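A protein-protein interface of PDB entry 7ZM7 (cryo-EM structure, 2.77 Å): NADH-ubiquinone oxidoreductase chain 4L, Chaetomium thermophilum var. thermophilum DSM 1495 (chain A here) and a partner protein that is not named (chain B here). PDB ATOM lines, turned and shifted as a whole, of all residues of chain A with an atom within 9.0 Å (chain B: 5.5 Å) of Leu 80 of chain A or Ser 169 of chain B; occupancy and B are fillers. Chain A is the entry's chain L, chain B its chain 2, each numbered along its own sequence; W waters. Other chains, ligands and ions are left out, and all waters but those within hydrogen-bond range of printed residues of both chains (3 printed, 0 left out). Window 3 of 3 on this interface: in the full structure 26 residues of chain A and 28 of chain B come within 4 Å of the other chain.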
ATOM      1  N   ILE A  73      21.253 -16.218  27.104  1.00  0.00           N
ATOM      2  CA  ILE A  73      22.034 -15.010  27.319  1.00  0.00           C
ATOM      3  C   ILE A  73      23.126 -14.900  26.271  1.00  0.00           C
ATOM      4  O   ILE A  73      23.451 -13.805  25.801  1.00  0.00           O
ATOM      5  CB  ILE A  73      22.600 -14.994  28.754  1.00  0.00           C
ATOM      6  CG1 ILE A  73      21.495 -14.678  29.752  1.00  0.00           C
ATOM      7  CG2 ILE A  73      23.714 -13.977  28.922  1.00  0.00           C
ATOM      8  CD1 ILE A  73      21.899 -14.868  31.173  1.00  0.00           C
ATOM      9  N   LEU A  74      23.722 -16.027  25.895  1.00  0.00           N
ATOM     10  CA  LEU A  74      24.729 -16.008  24.848  1.00  0.00           C
ATOM     11  C   LEU A  74      24.138 -15.606  23.501  1.00  0.00           C
ATOM     12  O   LEU A  74      24.851 -15.082  22.644  1.00  0.00           O
ATOM     13  CB  LEU A  74      25.400 -17.367  24.748  1.00  0.00           C
ATOM     14  CG  LEU A  74      26.523 -17.457  23.734  1.00  0.00           C
ATOM     15  CD1 LEU A  74      27.830 -17.040  24.357  1.00  0.00           C
ATOM     16  CD2 LEU A  74      26.589 -18.844  23.146  1.00  0.00           C
ATOM     17  N   VAL A  75      22.856 -15.881  23.275  1.00  0.00           N
ATOM     18  CA  VAL A  75      22.210 -15.409  22.058  1.00  0.00           C
ATOM     19  C   VAL A  75      22.031 -13.904  22.108  1.00  0.00           C
ATOM     20  O   VAL A  75      22.346 -13.195  21.150  1.00  0.00           O
ATOM     21  CB  VAL A  75      20.861 -16.120  21.841  1.00  0.00           C
ATOM     22  CG1 VAL A  75      20.009 -15.316  20.902  1.00  0.00           C
ATOM     23  CG2 VAL A  75      21.069 -17.492  21.299  1.00  0.00           C
ATOM     24  N   ALA A  76      21.562 -13.391  23.244  1.00  0.00           N
ATOM     25  CA  ALA A  76      21.354 -11.935  23.415  1.00  0.00           C
ATOM     26  C   ALA A  76      22.670 -11.187  23.182  1.00  0.00           C
ATOM     27  O   ALA A  76      22.644 -10.119  22.539  1.00  0.00           O
ATOM     28  CB  ALA A  76      20.805 -11.687  24.791  1.00  0.00           C
ATOM     29  N   PHE A  77      23.779 -11.729  23.678  1.00  0.00           N
ATOM     30  CA  PHE A  77      25.120 -11.125  23.497  1.00  0.00           C
ATOM     31  C   PHE A  77      25.507 -11.151  22.017  1.00  0.00           C
ATOM     32  O   PHE A  77      25.892 -10.097  21.496  1.00  0.00           O
ATOM     33  CB  PHE A  77      26.104 -11.847  24.422  1.00  0.00           C
ATOM     34  CG  PHE A  77      27.548 -11.435  24.309  1.00  0.00           C
ATOM     35  CD1 PHE A  77      28.007 -10.280  24.916  1.00  0.00           C
ATOM     36  CD2 PHE A  77      28.453 -12.220  23.616  1.00  0.00           C
ATOM     37  CE1 PHE A  77      29.336  -9.909  24.818  1.00  0.00           C
ATOM     38  CE2 PHE A  77      29.783 -11.850  23.520  1.00  0.00           C
ATOM     39  CZ  PHE A  77      30.221 -10.695  24.121  1.00  0.00           C
ATOM     40  N   TYR A  78      25.393 -12.304  21.357  1.00  0.00           N
ATOM     41  CA  TYR A  78      25.789 -12.464  19.932  1.00  0.00           C
ATOM     42  C   TYR A  78      25.005 -11.518  19.013  1.00  0.00           C
ATOM     43  O   TYR A  78      25.600 -11.041  18.049  1.00  0.00           O
ATOM     44  CB  TYR A  78      25.651 -13.935  19.531  1.00  0.00           C
ATOM     45  CG  TYR A  78      25.881 -14.239  18.074  1.00  0.00           C
ATOM     46  CD1 TYR A  78      27.159 -14.320  17.549  1.00  0.00           C
ATOM     47  CD2 TYR A  78      24.814 -14.461  17.225  1.00  0.00           C
ATOM     48  CE1 TYR A  78      27.370 -14.594  16.209  1.00  0.00           C
ATOM     49  CE2 TYR A  78      25.005 -14.738  15.884  1.00  0.00           C
ATOM     50  CZ  TYR A  78      26.287 -14.806  15.375  1.00  0.00           C
ATOM     51  OH  TYR A  78      26.465 -15.086  14.054  1.00  0.00           O
ATOM     52  N   ARG A  79      23.731 -11.254  19.296  1.00  0.00           N
ATOM     53  CA  ARG A  79      22.880 -10.409  18.422  1.00  0.00           C
ATOM     54  C   ARG A  79      23.518  -9.022  18.274  1.00  0.00           C
ATOM     55  O   ARG A  79      23.489  -8.479  17.159  1.00  0.00           O
ATOM     56  CB  ARG A  79      21.486 -10.262  19.043  1.00  0.00           C
ATOM     57  CG  ARG A  79      20.482  -9.534  18.164  1.00  0.00           C
ATOM     58  CD  ARG A  79      19.058  -9.709  18.644  1.00  0.00           C
ATOM     59  NE  ARG A  79      18.828  -8.850  19.787  1.00  0.00           N
ATOM     60  CZ  ARG A  79      18.218  -7.676  19.733  1.00  0.00           C
ATOM     61  NH1 ARG A  79      18.073  -6.967  20.834  1.00  0.00           N
ATOM     62  NH2 ARG A  79      17.730  -7.226  18.593  1.00  0.00           N
ATOM     63  N   LEU A  80      24.064  -8.471  19.363  1.00  0.00           N
ATOM     64  CA  LEU A  80      24.689  -7.128  19.315  1.00  0.00           C
ATOM     65  C   LEU A  80      26.194  -7.201  19.048  1.00  0.00           C
ATOM     66  O   LEU A  80      26.764  -6.164  18.703  1.00  0.00           O
ATOM     67  CB  LEU A  80      24.381  -6.399  20.624  1.00  0.00           C
ATOM     68  CG  LEU A  80      22.942  -6.529  21.118  1.00  0.00           C
ATOM     69  CD1 LEU A  80      22.794  -5.942  22.510  1.00  0.00           C
ATOM     70  CD2 LEU A  80      21.972  -5.868  20.155  1.00  0.00           C
ATOM     71  N   ARG A  81      26.791  -8.420  19.208  1.00  0.00           N
ATOM     72  CA  ARG A  81      28.269  -8.494  19.074  1.00  0.00           C
ATOM     73  C   ARG A  81      28.636  -9.026  17.684  1.00  0.00           C
ATOM     74  O   ARG A  81      29.439  -8.369  17.005  1.00  0.00           O
ATOM     75  CB  ARG A  81      28.875  -9.281  20.240  1.00  0.00           C
ATOM     76  CG  ARG A  81      30.384  -9.162  20.377  1.00  0.00           C
ATOM     77  CD  ARG A  81      30.799  -8.059  21.324  1.00  0.00           C
ATOM     78  NE  ARG A  81      32.117  -8.317  21.882  1.00  0.00           N
ATOM     79  CZ  ARG A  81      32.791  -7.469  22.649  1.00  0.00           C
ATOM     80  NH1 ARG A  81      32.274  -6.288  22.941  1.00  0.00           N
ATOM     81  NH2 ARG A  81      33.984  -7.799  23.109  1.00  0.00           N
ATOM     82  N   GLY A  82      28.059 -10.107  17.244  1.00  0.00           N
ATOM     83  CA  GLY A  82      28.419 -10.749  15.963  1.00  0.00           C
ATOM     84  C   GLY A  82      29.610 -11.655  16.103  1.00  0.00           C
ATOM     85  O   GLY A  82      30.107 -12.121  15.078  1.00  0.00           O
ATOM     86  N   SER A  83      30.038 -11.900  17.337  1.00  0.00           N
ATOM     87  CA  SER A  83      31.232 -12.735  17.594  1.00  0.00           C
ATOM     88  C   SER A  83      31.195 -13.221  19.041  1.00  0.00           C
ATOM     89  O   SER A  83      30.794 -12.438  19.910  1.00  0.00           O
ATOM     90  CB  SER A  83      32.481 -11.970  17.315  1.00  0.00           C
ATOM     91  OG  SER A  83      33.609 -12.828  17.337  1.00  0.00           O
ATOM     92  N   TYR B 166      17.875  -5.648  29.739  1.00  0.00           N
ATOM     93  CA  TYR B 166      17.956  -4.521  28.784  1.00  0.00           C
ATOM     94  C   TYR B 166      18.591  -5.195  27.580  1.00  0.00           C
ATOM     95  O   TYR B 166      19.822  -5.243  27.514  1.00  0.00           O
ATOM     96  CB  TYR B 166      18.586  -3.286  29.427  1.00  0.00           C
ATOM     97  CG  TYR B 166      17.698  -2.588  30.423  1.00  0.00           C
ATOM     98  CD1 TYR B 166      17.437  -3.155  31.657  1.00  0.00           C
ATOM     99  CD2 TYR B 166      17.130  -1.357  30.142  1.00  0.00           C
ATOM    100  CE1 TYR B 166      16.634  -2.524  32.588  1.00  0.00           C
ATOM    101  CE2 TYR B 166      16.327  -0.708  31.062  1.00  0.00           C
ATOM    102  CZ  TYR B 166      16.080  -1.294  32.290  1.00  0.00           C
ATOM    103  OH  TYR B 166      15.294  -0.683  33.217  1.00  0.00           O
ATOM    104  N   ARG B 167      17.762  -5.760  26.700  1.00  0.00           N
ATOM    105  CA  ARG B 167      18.256  -6.625  25.595  1.00  0.00           C
ATOM    106  C   ARG B 167      18.929  -5.812  24.503  1.00  0.00           C
ATOM    107  O   ARG B 167      19.662  -6.400  23.707  1.00  0.00           O
ATOM    108  CB  ARG B 167      17.095  -7.478  25.076  1.00  0.00           C
ATOM    109  CG  ARG B 167      15.853  -6.705  24.662  1.00  0.00           C
ATOM    110  CD  ARG B 167      14.782  -7.692  24.237  1.00  0.00           C
ATOM    111  NE  ARG B 167      15.272  -8.618  23.228  1.00  0.00           N
ATOM    112  CZ  ARG B 167      15.135  -8.455  21.918  1.00  0.00           C
ATOM    113  NH1 ARG B 167      15.626  -9.359  21.091  1.00  0.00           N
ATOM    114  NH2 ARG B 167      14.505  -7.400  21.438  1.00  0.00           N
ATOM    115  N   ASN B 168      18.724  -4.507  24.502  1.00  0.00           N
ATOM    116  CA  ASN B 168      19.246  -3.708  23.413  1.00  0.00           C
ATOM    117  C   ASN B 168      20.479  -2.916  23.807  1.00  0.00           C
ATOM    118  O   ASN B 168      20.895  -2.027  23.065  1.00  0.00           O
ATOM    119  CB  ASN B 168      18.148  -2.806  22.866  1.00  0.00           C
ATOM    120  CG  ASN B 168      17.153  -3.571  22.041  1.00  0.00           C
ATOM    121  OD1 ASN B 168      17.459  -4.642  21.553  1.00  0.00           O
ATOM    122  ND2 ASN B 168      15.964  -3.045  21.894  1.00  0.00           N
ATOM    123  N   SER B 169      21.085  -3.241  24.942  1.00  0.00           N
ATOM    124  CA  SER B 169      22.334  -2.646  25.386  1.00  0.00           C
ATOM    125  C   SER B 169      23.458  -3.664  25.258  1.00  0.00           C
ATOM    126  O   SER B 169      23.348  -4.783  25.757  1.00  0.00           O
ATOM    127  CB  SER B 169      22.222  -2.181  26.827  1.00  0.00           C
ATOM    128  OG  SER B 169      21.081  -1.373  26.973  1.00  0.00           O
ATOM    129  N   GLU B 170      24.529  -3.271  24.571  1.00  0.00           N
ATOM    130  CA  GLU B 170      25.713  -4.113  24.496  1.00  0.00           C
ATOM    131  C   GLU B 170      26.341  -4.284  25.865  1.00  0.00           C
ATOM    132  O   GLU B 170      26.912  -5.337  26.170  1.00  0.00           O
ATOM    133  CB  GLU B 170      26.714  -3.506  23.528  1.00  0.00           C
ATOM    134  CG  GLU B 170      26.218  -3.437  22.114  1.00  0.00           C
ATOM    135  CD  GLU B 170      27.198  -2.763  21.182  1.00  0.00           C
ATOM    136  OE1 GLU B 170      27.598  -1.610  21.448  1.00  0.00           O
ATOM    137  OE2 GLU B 170      27.573  -3.393  20.180  1.00  0.00           O
ATOM    138  N   LEU B 171      26.244  -3.260  26.711  1.00  0.00           N
ATOM    139  CA  LEU B 171      26.785  -3.370  28.059  1.00  0.00           C
ATOM    140  C   LEU B 171      26.003  -4.360  28.898  1.00  0.00           C
ATOM    141  O   LEU B 171      26.592  -5.221  29.553  1.00  0.00           O
ATOM    142  CB  LEU B 171      26.783  -2.013  28.738  1.00  0.00           C
ATOM    143  CG  LEU B 171      27.729  -0.989  28.162  1.00  0.00           C
ATOM    144  CD1 LEU B 171      27.662   0.196  29.064  1.00  0.00           C
ATOM    145  CD2 LEU B 171      29.109  -1.571  28.086  1.00  0.00           C
ATOM    146  N   SER B 172      24.678  -4.250  28.898  1.00  0.00           N
ATOM    147  CA  SER B 172      23.879  -5.085  29.783  1.00  0.00           C
ATOM    148  C   SER B 172      24.010  -6.553  29.435  1.00  0.00           C
ATOM    149  O   SER B 172      24.076  -7.401  30.324  1.00  0.00           O
ATOM    150  CB  SER B 172      22.417  -4.649  29.751  1.00  0.00           C
ATOM    151  OG  SER B 172      22.266  -3.397  30.369  1.00  0.00           O
ATOM    152  N   THR B 173      24.025  -6.877  28.151  1.00  0.00           N
ATOM    153  CA  THR B 173      24.116  -8.275  27.751  1.00  0.00           C
ATOM    154  C   THR B 173      25.497  -8.834  28.032  1.00  0.00           C
ATOM    155  O   THR B 173      25.638 -10.016  28.334  1.00  0.00           O
ATOM    156  CB  THR B 173      23.751  -8.417  26.272  1.00  0.00           C
ATOM    157  OG1 THR B 173      24.572  -7.544  25.501  1.00  0.00           O
ATOM    158  CG2 THR B 173      22.318  -8.043  26.049  1.00  0.00           C
ATOM    159  N   THR B 174      26.519  -7.988  27.945  1.00  0.00           N
ATOM    160  CA  THR B 174      27.868  -8.373  28.335  1.00  0.00           C
ATOM    161  C   THR B 174      27.946  -8.694  29.816  1.00  0.00           C
ATOM    162  O   THR B 174      28.569  -9.684  30.212  1.00  0.00           O
ATOM    163  CB  THR B 174      28.821  -7.243  27.991  1.00  0.00           C
ATOM    164  OG1 THR B 174      28.877  -7.102  26.572  1.00  0.00           O
ATOM    165  CG2 THR B 174      30.183  -7.506  28.533  1.00  0.00           C
ATOM    166  N   ASP B 406      25.506   3.952  26.772  1.00  0.00           N
ATOM    167  CA  ASP B 406      24.252   3.698  27.529  1.00  0.00           C
ATOM    168  C   ASP B 406      23.980   4.895  28.429  1.00  0.00           C
ATOM    169  O   ASP B 406      23.736   4.682  29.627  1.00  0.00           O
ATOM    170  CB  ASP B 406      24.304   2.406  28.340  1.00  0.00           C
ATOM    171  CG  ASP B 406      24.264   1.130  27.518  1.00  0.00           C
ATOM    172  OD1 ASP B 406      24.463   1.209  26.290  1.00  0.00           O
ATOM    173  OD2 ASP B 406      24.028   0.066  28.117  1.00  0.00           O
ATOM    174  N   ASN B 409      20.716   4.254  30.291  1.00  0.00           N
ATOM    175  CA  ASN B 409      20.647   3.213  31.305  1.00  0.00           C
ATOM    176  C   ASN B 409      21.477   3.554  32.531  1.00  0.00           C
ATOM    177  O   ASN B 409      21.127   3.157  33.641  1.00  0.00           O
ATOM    178  CB  ASN B 409      21.110   1.882  30.722  1.00  0.00           C
ATOM    179  CG  ASN B 409      20.351   1.501  29.494  1.00  0.00           C
ATOM    180  OD1 ASN B 409      20.938   1.196  28.460  1.00  0.00           O
ATOM    181  ND2 ASN B 409      19.029   1.534  29.585  1.00  0.00           N
HETATM  182  O   HOH W   1      29.885  -6.079  24.358  1.00  0.00           O
HETATM  183  O   HOH W   2      26.396  -7.548  23.023  1.00  0.00           O
HETATM  184  O   HOH W   3      19.669  -8.790  22.530  1.00  0.00           O
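The guanidinium group (NH1) of Arg 79 of chain A is in hydrogen-bond range of the backbone carbonyl oxygen (O) of Arg 167 of chain B, at 3.3 Å.
OD1 of Asn 168 of chain B is in hydrogen-bond range of NH1 of Arg 79 of chain A.
The backbone carbonyl oxygen of Leu 80 of chain A lies close to the side-chain carboxylate of Glu 170 of chain B, 3.2 Å away.
O of Ser 169 of chain B sits at hydrogen-bond distance from OG1 of Thr 173 of chain B (3.0 Å).
The side-chain hydroxyl of Thr 173 of chain B lies within hydrogen-bond range of the backbone carbonyl oxygen of Glu 170 of chain B, at 3.3 Å.
The side-chain hydroxyl of Ser 169 of chain B is in hydrogen-bond range of the side-chain amide oxygen of Asn 409 of chain B (3.0 Å).
The side-chain hydroxyl of Thr 174 of chain B sits at hydrogen-bond distance from the backbone carbonyl oxygen of Glu 170 of chain B (2.7 Å).
The side-chain hydroxyl of Ser 169 of chain B sits close to the side-chain carboxylate of Asp 406 of chain B (3.5 Å).
Leu 80 of chain A touches four residues of chain B.
Of the printed residues of chain A, Glu 170 of chain B touches Leu 80 (3.2 Å).
Of the printed residues of chain B, Arg 79 of chain A touches Arg 167 (3.3 Å) and Asn 168 (2.5 Å).
Printed residues of chain A within 4 Å of Thr 174 of chain B: Phe 77.
Printed residues of chain A within 4 Å of Thr 173 of chain B: Leu 80 (3.8 Å).
Printed residues of chain B within 4 Å of Phe 77 of chain A: Thr 174.
Ala 76 of chain A touches none of the printed residues of chain B.
The nearest printed residue of chain A that does not touch Thr 174 of chain B is Arg 81 of chain A (5.0 Å).
Water W1 lies within hydrogen-bond range of OG1 of Thr 174 of chain B and NH1 of Arg 81 of chain A.
Water W3 lies within hydrogen-bond range of the backbone carbonyl oxygen of Arg 167 of chain B (2.7 Å), the guanidinium group of Arg 79 of chain A (2.9 Å) and the backbone carbonyl oxygen of Ala 76 of chain A (3.3 Å).
Water W2 bridges O of Phe 77 of chain A and OG1 of Thr 173 of chain B.
OG1 of Thr 174 of chain B touches CE1 of Phe 77 of chain A, 3.3 Å away.
Leu 80 of chain A touches Arg 167 of chain B.
Ser 169 of chain B touches Leu 80 of chain A (O to CD1, 3.5 Å).
CD1 of Leu 80 of chain A touches OG1 of Thr 173 of chain B (3.8 Å).
Of the 11 printed residues of chain A, 3 touch a printed residue of chain B.
Hydrophobic or aromatic side chains of chain A within 4 Å of the printed part of chain B: Phe 77 and Leu 80.
Among the printed residues, 7 pairs touch across the chains.
Among the printed residues, no Asp or Glu carboxylate lies within 4 Å of a Lys or Arg side-chain nitrogen of the other chain.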
